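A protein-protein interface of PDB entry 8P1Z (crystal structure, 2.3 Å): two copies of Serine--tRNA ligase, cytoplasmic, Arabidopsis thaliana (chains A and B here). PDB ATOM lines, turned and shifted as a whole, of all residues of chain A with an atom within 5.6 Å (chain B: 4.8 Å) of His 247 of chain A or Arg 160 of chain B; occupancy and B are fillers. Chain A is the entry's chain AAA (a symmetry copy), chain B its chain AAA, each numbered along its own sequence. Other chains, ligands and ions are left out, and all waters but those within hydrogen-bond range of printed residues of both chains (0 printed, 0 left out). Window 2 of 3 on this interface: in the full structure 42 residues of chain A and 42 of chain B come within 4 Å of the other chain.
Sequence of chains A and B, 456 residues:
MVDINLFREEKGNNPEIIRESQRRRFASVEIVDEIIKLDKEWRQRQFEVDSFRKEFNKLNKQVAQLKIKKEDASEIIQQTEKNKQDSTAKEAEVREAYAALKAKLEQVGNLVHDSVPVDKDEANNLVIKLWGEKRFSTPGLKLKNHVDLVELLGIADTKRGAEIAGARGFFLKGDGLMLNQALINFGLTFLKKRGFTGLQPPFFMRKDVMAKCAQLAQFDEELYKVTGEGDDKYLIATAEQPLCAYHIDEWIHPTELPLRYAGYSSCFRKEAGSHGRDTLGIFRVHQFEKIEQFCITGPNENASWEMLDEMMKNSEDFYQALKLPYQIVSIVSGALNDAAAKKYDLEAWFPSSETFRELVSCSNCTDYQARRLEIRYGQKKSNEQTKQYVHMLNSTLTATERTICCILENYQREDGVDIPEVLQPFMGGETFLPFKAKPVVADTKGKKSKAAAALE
The side-chain carboxylate (OD2) of Asp 157 of chain B is in hydrogen-bond range of the side-chain hydroxyl (OH) of Tyr 246 of chain A, at 3.3 Å.
The guanidinium group of Arg 160 of chain B is in hydrogen-bond range of the side-chain hydroxyl of Tyr 246 of chain A (3.2 Å).
The side-chain carboxylate of Glu 250 of chain A is in salt-bridge range of the guanidinium group of Arg 160 of chain B (2.6 Å).
OD1 of Asp 157 of chain B sits at hydrogen-bond distance from N of Lys 159 of chain B.
The guanidinium group (NH1) of Arg 160 of chain B is in salt-bridge range of the side-chain carboxylate (OD2) of Asp 157 of chain B, 2.8 Å away.
O of Asp 157 of chain B sits at hydrogen-bond distance from N of Phe 171 of chain B (3.1 Å).
A ring nitrogen (ND1) of His 247 of chain A sits at hydrogen-bond distance from the side-chain carboxylate of Glu 250 of chain A (3.0 Å).
A ring nitrogen (NE2) of His 247 of chain A is in hydrogen-bond range of the side-chain hydroxyl of Tyr 261 of chain A (2.7 Å).
Among the printed residues, merely in contact across the chains: Ala 245 of chain A with Ile 164 of chain B, His 247 of chain A with Arg 160 of chain B, Tyr 246 of chain A with Phe 171 of chain B and Tyr 246 of chain A with Ile 164 of chain B.
Of the printed residues of chain B, Tyr 246 of chain A touches Asp 157, Arg 160, Ile 164 and Phe 171.
His 247 of chain A touches just one residue of chain B: Arg 160.
Of the printed residues of chain B, Glu 250 of chain A touches Arg 160.
Arg 160 of chain B touches just these residues of chain A: Tyr 246 (3.2 Å), His 247 (3.6 Å) and Glu 250 (2.6 Å).
Glu 163 of chain B touches none of the printed residues of chain A.
Printed residues of chain A within 4 Å of Ile 164 of chain B: Ala 245 and Tyr 246.
Of the printed residues of chain A, Phe 171 of chain B touches Tyr 246.
The nearest printed residue of chain A that does not touch Phe 171 of chain B is Ala 245 of chain A (6.2 Å).
Of the 14 printed residues of chain A, 4 touch a printed residue of chain B.
Of the 9 printed residues of chain B, 4 touch a printed residue of chain A.
Among the printed residues, 7 pairs touch across the chains.
No position is printed for both chains.
Of the 7 pairs that touch across the chains among the printed residues, none has its exchanged pair printed and touching as well.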
ATOM      1  N   CYS A 244       4.575  -0.359  29.913  1.00  0.00           N
ATOM      2  CA  CYS A 244       3.315  -1.064  30.256  1.00  0.00           C
ATOM      3  C   CYS A 244       2.669  -1.365  28.898  1.00  0.00           C
ATOM      4  O   CYS A 244       2.451  -2.557  28.609  1.00  0.00           O
ATOM      5  CB  CYS A 244       2.507  -0.230  31.254  1.00  0.00           C
ATOM      6  SG  CYS A 244       0.739  -0.611  31.427  1.00  0.00           S
ATOM      7  N   ALA A 245       2.536  -0.343  28.040  1.00  0.00           N
ATOM      8  CA  ALA A 245       2.224  -0.503  26.599  1.00  0.00           C
ATOM      9  C   ALA A 245       3.323  -1.344  25.935  1.00  0.00           C
ATOM     10  O   ALA A 245       2.967  -2.234  25.156  1.00  0.00           O
ATOM     11  CB  ALA A 245       2.076   0.832  25.927  1.00  0.00           C
ATOM     12  N   TYR A 246       4.604  -1.100  26.244  1.00  0.00           N
ATOM     13  CA  TYR A 246       5.740  -1.957  25.799  1.00  0.00           C
ATOM     14  C   TYR A 246       5.429  -3.376  26.258  1.00  0.00           C
ATOM     15  O   TYR A 246       5.193  -3.532  27.484  1.00  0.00           O
ATOM     16  CB  TYR A 246       7.059  -1.498  26.424  1.00  0.00           C
ATOM     17  CG  TYR A 246       8.354  -2.059  25.874  1.00  0.00           C
ATOM     18  CD1 TYR A 246       8.807  -3.335  26.180  1.00  0.00           C
ATOM     19  CD2 TYR A 246       9.209  -1.247  25.146  1.00  0.00           C
ATOM     20  CE1 TYR A 246      10.033  -3.804  25.727  1.00  0.00           C
ATOM     21  CE2 TYR A 246      10.430  -1.698  24.674  1.00  0.00           C
ATOM     22  CZ  TYR A 246      10.850  -2.981  24.966  1.00  0.00           C
ATOM     23  OH  TYR A 246      12.061  -3.391  24.471  1.00  0.00           O
ATOM     24  N   HIS A 247       5.432  -4.336  25.328  1.00  0.00           N
ATOM     25  CA  HIS A 247       5.103  -5.783  25.518  1.00  0.00           C
ATOM     26  C   HIS A 247       3.603  -6.048  25.359  1.00  0.00           C
ATOM     27  O   HIS A 247       3.222  -7.184  25.648  1.00  0.00           O
ATOM     28  CB  HIS A 247       5.583  -6.373  26.853  1.00  0.00           C
ATOM     29  CG  HIS A 247       7.043  -6.671  26.924  1.00  0.00           C
ATOM     30  ND1 HIS A 247       7.762  -7.176  25.848  1.00  0.00           N
ATOM     31  CD2 HIS A 247       7.916  -6.557  27.949  1.00  0.00           C
ATOM     32  CE1 HIS A 247       9.020  -7.345  26.207  1.00  0.00           C
ATOM     33  NE2 HIS A 247       9.139  -6.973  27.495  1.00  0.00           N
ATOM     34  N   ILE A 248       2.806  -5.080  24.878  1.00  0.00           N
ATOM     35  CA  ILE A 248       1.365  -5.281  24.514  1.00  0.00           C
ATOM     36  C   ILE A 248       1.210  -6.418  23.491  1.00  0.00           C
ATOM     37  O   ILE A 248       1.987  -6.472  22.521  1.00  0.00           O
ATOM     38  CB  ILE A 248       0.741  -3.991  23.958  1.00  0.00           C
ATOM     39  CG1 ILE A 248      -0.771  -4.131  23.768  1.00  0.00           C
ATOM     40  CG2 ILE A 248       1.423  -3.576  22.665  1.00  0.00           C
ATOM     41  CD1 ILE A 248      -1.492  -2.810  23.574  1.00  0.00           C
ATOM     42  N   ASP A 249       0.198  -7.265  23.682  1.00  0.00           N
ATOM     43  CA  ASP A 249      -0.160  -8.374  22.761  1.00  0.00           C
ATOM     44  C   ASP A 249       0.988  -9.373  22.610  1.00  0.00           C
ATOM     45  O   ASP A 249       0.898 -10.209  21.713  1.00  0.00           O
ATOM     46  CB  ASP A 249      -0.556  -7.851  21.379  1.00  0.00           C
ATOM     47  CG  ASP A 249      -2.046  -7.607  21.271  1.00  0.00           C
ATOM     48  OD1 ASP A 249      -2.816  -8.507  21.692  1.00  0.00           O
ATOM     49  OD2 ASP A 249      -2.424  -6.523  20.780  1.00  0.00           O
ATOM     50  N   GLU A 250       2.003  -9.344  23.462  1.00  0.00           N
ATOM     51  CA  GLU A 250       3.158 -10.254  23.291  1.00  0.00           C
ATOM     52  C   GLU A 250       3.006 -11.452  24.221  1.00  0.00           C
ATOM     53  O   GLU A 250       2.275 -11.362  25.208  1.00  0.00           O
ATOM     54  CB  GLU A 250       4.468  -9.525  23.561  1.00  0.00           C
ATOM     55  CG  GLU A 250       4.604  -8.230  22.788  1.00  0.00           C
ATOM     56  CD  GLU A 250       6.017  -7.681  22.814  1.00  0.00           C
ATOM     57  OE1 GLU A 250       6.215  -6.509  22.406  1.00  0.00           O
ATOM     58  OE2 GLU A 250       6.917  -8.431  23.260  1.00  0.00           O
ATOM     59  N   ILE A 252       5.423 -13.683  26.735  1.00  0.00           N
ATOM     60  CA  ILE A 252       6.755 -13.675  27.386  1.00  0.00           C
ATOM     61  C   ILE A 252       6.977 -15.094  27.890  1.00  0.00           C
ATOM     62  O   ILE A 252       6.028 -15.667  28.463  1.00  0.00           O
ATOM     63  CB  ILE A 252       6.860 -12.562  28.457  1.00  0.00           C
ATOM     64  CG1 ILE A 252       6.545 -11.199  27.821  1.00  0.00           C
ATOM     65  CG2 ILE A 252       8.226 -12.582  29.157  1.00  0.00           C
ATOM     66  CD1 ILE A 252       6.863  -9.992  28.673  1.00  0.00           C
ATOM     67  N   LEU A 259      11.652  -9.772  34.287  1.00  0.00           N
ATOM     68  CA  LEU A 259      12.220  -8.655  33.509  1.00  0.00           C
ATOM     69  C   LEU A 259      12.387  -7.447  34.428  1.00  0.00           C
ATOM     70  O   LEU A 259      11.443  -7.120  35.149  1.00  0.00           O
ATOM     71  CB  LEU A 259      11.271  -8.356  32.349  1.00  0.00           C
ATOM     72  CG  LEU A 259      11.329  -9.359  31.199  1.00  0.00           C
ATOM     73  CD1 LEU A 259      10.296  -9.020  30.136  1.00  0.00           C
ATOM     74  CD2 LEU A 259      12.724  -9.393  30.591  1.00  0.00           C
ATOM     75  N   TYR A 261      13.371  -3.437  34.120  1.00  0.00           N
ATOM     76  CA  TYR A 261      13.622  -2.191  33.364  1.00  0.00           C
ATOM     77  C   TYR A 261      13.779  -1.004  34.320  1.00  0.00           C
ATOM     78  O   TYR A 261      12.871  -0.757  35.170  1.00  0.00           O
ATOM     79  CB  TYR A 261      12.457  -1.918  32.417  1.00  0.00           C
ATOM     80  CG  TYR A 261      12.171  -3.015  31.429  1.00  0.00           C
ATOM     81  CD1 TYR A 261      13.187  -3.600  30.696  1.00  0.00           C
ATOM     82  CD2 TYR A 261      10.872  -3.418  31.173  1.00  0.00           C
ATOM     83  CE1 TYR A 261      12.927  -4.588  29.761  1.00  0.00           C
ATOM     84  CE2 TYR A 261      10.594  -4.405  30.244  1.00  0.00           C
ATOM     85  CZ  TYR A 261      11.626  -4.994  29.532  1.00  0.00           C
ATOM     86  OH  TYR A 261      11.366  -5.967  28.609  1.00  0.00           O
ATOM     87  N   ILE A 296       8.393  -7.145  35.406  1.00  0.00           N
ATOM     88  CA  ILE A 296       7.428  -8.201  35.006  1.00  0.00           C
ATOM     89  C   ILE A 296       7.890  -9.502  35.635  1.00  0.00           C
ATOM     90  O   ILE A 296       9.104  -9.750  35.627  1.00  0.00           O
ATOM     91  CB  ILE A 296       7.292  -8.311  33.482  1.00  0.00           C
ATOM     92  CG1 ILE A 296       6.971  -6.947  32.880  1.00  0.00           C
ATOM     93  CG2 ILE A 296       6.244  -9.364  33.137  1.00  0.00           C
ATOM     94  CD1 ILE A 296       6.764  -6.959  31.392  1.00  0.00           C
ATOM     95  N   LEU A 373      -3.961  -5.744  28.321  1.00  0.00           N
ATOM     96  CA  LEU A 373      -2.896  -5.549  27.300  1.00  0.00           C
ATOM     97  C   LEU A 373      -2.532  -6.882  26.636  1.00  0.00           C
ATOM     98  O   LEU A 373      -1.586  -6.909  25.831  1.00  0.00           O
ATOM     99  CB  LEU A 373      -1.690  -4.922  27.998  1.00  0.00           C
ATOM    100  CG  LEU A 373      -1.965  -3.570  28.654  1.00  0.00           C
ATOM    101  CD1 LEU A 373      -0.850  -3.199  29.613  1.00  0.00           C
ATOM    102  CD2 LEU A 373      -2.139  -2.481  27.611  1.00  0.00           C
ATOM    103  N   GLU A 374      -3.252  -7.950  26.962  1.00  0.00           N
ATOM    104  CA  GLU A 374      -3.014  -9.300  26.409  1.00  0.00           C
ATOM    105  C   GLU A 374      -1.514  -9.586  26.440  1.00  0.00           C
ATOM    106  O   GLU A 374      -0.964  -9.959  25.407  1.00  0.00           O
ATOM    107  CB  GLU A 374      -3.649  -9.383  25.022  1.00  0.00           C
ATOM    108  CG  GLU A 374      -5.095  -9.835  25.079  1.00  0.00           C
ATOM    109  CD  GLU A 374      -5.292 -11.198  25.738  1.00  0.00           C
ATOM    110  OE1 GLU A 374      -4.462 -12.108  25.487  1.00  0.00           O
ATOM    111  OE2 GLU A 374      -6.253 -11.349  26.517  1.00  0.00           O
ATOM    112  N   ILE A 375      -0.896  -9.415  27.606  1.00  0.00           N
ATOM    113  CA  ILE A 375       0.532  -9.752  27.880  1.00  0.00           C
ATOM    114  C   ILE A 375       0.566 -11.103  28.600  1.00  0.00           C
ATOM    115  O   ILE A 375       0.299 -11.138  29.820  1.00  0.00           O
ATOM    116  CB  ILE A 375       1.210  -8.623  28.676  1.00  0.00           C
ATOM    117  CG1 ILE A 375       0.881  -7.259  28.065  1.00  0.00           C
ATOM    118  CG2 ILE A 375       2.707  -8.845  28.771  1.00  0.00           C
ATOM    119  CD1 ILE A 375       1.366  -6.073  28.866  1.00  0.00           C
ATOM    120  N   ASP B 157      14.266   0.480  20.559  1.00  0.00           N
ATOM    121  CA  ASP B 157      13.055  -0.187  20.037  1.00  0.00           C
ATOM    122  C   ASP B 157      12.266   0.860  19.267  1.00  0.00           C
ATOM    123  O   ASP B 157      11.502   1.609  19.901  1.00  0.00           O
ATOM    124  CB  ASP B 157      12.231  -0.870  21.126  1.00  0.00           C
ATOM    125  CG  ASP B 157      11.464  -2.059  20.575  1.00  0.00           C
ATOM    126  OD1 ASP B 157      10.832  -1.895  19.495  1.00  0.00           O
ATOM    127  OD2 ASP B 157      11.531  -3.144  21.212  1.00  0.00           O
ATOM    128  N   THR B 158      12.481   0.916  17.954  1.00  0.00           N
ATOM    129  CA  THR B 158      11.728   1.795  17.029  1.00  0.00           C
ATOM    130  C   THR B 158      10.354   1.181  16.731  1.00  0.00           C
ATOM    131  O   THR B 158       9.442   1.957  16.412  1.00  0.00           O
ATOM    132  CB  THR B 158      12.530   2.074  15.753  1.00  0.00           C
ATOM    133  OG1 THR B 158      12.926   0.827  15.175  1.00  0.00           O
ATOM    134  CG2 THR B 158      13.749   2.925  16.021  1.00  0.00           C
ATOM    135  N   LYS B 159      10.215  -0.146  16.807  1.00  0.00           N
ATOM    136  CA  LYS B 159       8.955  -0.855  16.447  1.00  0.00           C
ATOM    137  C   LYS B 159       7.934  -0.611  17.561  1.00  0.00           C
ATOM    138  O   LYS B 159       6.858  -0.064  17.272  1.00  0.00           O
ATOM    139  CB  LYS B 159       9.192  -2.354  16.195  1.00  0.00           C
ATOM    140  CG  LYS B 159       9.348  -2.750  14.728  1.00  0.00           C
ATOM    141  CD  LYS B 159      10.169  -4.017  14.488  1.00  0.00           C
ATOM    142  CE  LYS B 159       9.648  -5.241  15.214  1.00  0.00           C
ATOM    143  N   ARG B 160       8.284  -0.994  18.791  1.00  0.00           N
ATOM    144  CA  ARG B 160       7.443  -0.818  20.003  1.00  0.00           C
ATOM    145  C   ARG B 160       7.256   0.687  20.256  1.00  0.00           C
ATOM    146  O   ARG B 160       6.137   1.118  20.599  1.00  0.00           O
ATOM    147  CB  ARG B 160       8.074  -1.559  21.186  1.00  0.00           C
ATOM    148  CG  ARG B 160       8.018  -3.078  21.084  1.00  0.00           C
ATOM    149  CD  ARG B 160       8.448  -3.717  22.392  1.00  0.00           C
ATOM    150  NE  ARG B 160       8.407  -5.180  22.447  1.00  0.00           N
ATOM    151  CZ  ARG B 160       9.471  -5.990  22.528  1.00  0.00           C
ATOM    152  NH1 ARG B 160      10.702  -5.502  22.533  1.00  0.00           N
ATOM    153  NH2 ARG B 160       9.303  -7.298  22.605  1.00  0.00           N
ATOM    154  N   GLY B 161       8.304   1.474  20.059  1.00  0.00           N
ATOM    155  CA  GLY B 161       8.191   2.939  20.046  1.00  0.00           C
ATOM    156  C   GLY B 161       7.045   3.393  19.158  1.00  0.00           C
ATOM    157  O   GLY B 161       6.290   4.281  19.588  1.00  0.00           O
ATOM    158  N   ALA B 162       6.911   2.807  17.965  1.00  0.00           N
ATOM    159  CA  ALA B 162       5.996   3.300  16.904  1.00  0.00           C
ATOM    160  C   ALA B 162       4.546   2.997  17.291  1.00  0.00           C
ATOM    161  O   ALA B 162       3.711   3.902  17.144  1.00  0.00           O
ATOM    162  CB  ALA B 162       6.351   2.723  15.552  1.00  0.00           C
ATOM    163  N   GLU B 163       4.262   1.784  17.775  1.00  0.00           N
ATOM    164  CA  GLU B 163       2.920   1.402  18.305  1.00  0.00           C
ATOM    165  C   GLU B 163       2.517   2.364  19.441  1.00  0.00           C
ATOM    166  O   GLU B 163       1.339   2.780  19.467  1.00  0.00           O
ATOM    167  CB  GLU B 163       2.907  -0.049  18.798  1.00  0.00           C
ATOM    168  CG  GLU B 163       3.098  -1.086  17.705  1.00  0.00           C
ATOM    169  CD  GLU B 163       3.582  -2.437  18.220  1.00  0.00           C
ATOM    170  OE1 GLU B 163       2.744  -3.238  18.711  1.00  0.00           O
ATOM    171  OE2 GLU B 163       4.807  -2.678  18.161  1.00  0.00           O
ATOM    172  N   ILE B 164       3.467   2.719  20.321  1.00  0.00           N
ATOM    173  CA  ILE B 164       3.257   3.557  21.543  1.00  0.00           C
ATOM    174  C   ILE B 164       3.079   5.043  21.153  1.00  0.00           C
ATOM    175  O   ILE B 164       2.053   5.629  21.548  1.00  0.00           O
ATOM    176  CB  ILE B 164       4.407   3.331  22.558  1.00  0.00           C
ATOM    177  CG1 ILE B 164       4.154   2.130  23.475  1.00  0.00           C
ATOM    178  CG2 ILE B 164       4.682   4.580  23.386  1.00  0.00           C
ATOM    179  CD1 ILE B 164       4.256   0.782  22.808  1.00  0.00           C
ATOM    180  N   PHE B 171      12.085   4.020  21.711  1.00  0.00           N
ATOM    181  CA  PHE B 171      12.748   3.861  23.030  1.00  0.00           C
ATOM    182  C   PHE B 171      14.265   3.892  22.831  1.00  0.00           C
ATOM    183  O   PHE B 171      14.714   3.329  21.846  1.00  0.00           O
ATOM    184  CB  PHE B 171      12.350   2.533  23.670  1.00  0.00           C
ATOM    185  CG  PHE B 171      10.911   2.434  24.106  1.00  0.00           C
ATOM    186  CD1 PHE B 171       9.897   2.256  23.178  1.00  0.00           C
ATOM    187  CD2 PHE B 171      10.571   2.501  25.449  1.00  0.00           C
ATOM    188  CE1 PHE B 171       8.575   2.154  23.584  1.00  0.00           C
ATOM    189  CE2 PHE B 171       9.251   2.382  25.852  1.00  0.00           C
ATOM    190  CZ  PHE B 171       8.256   2.214  24.920  1.00  0.00           C
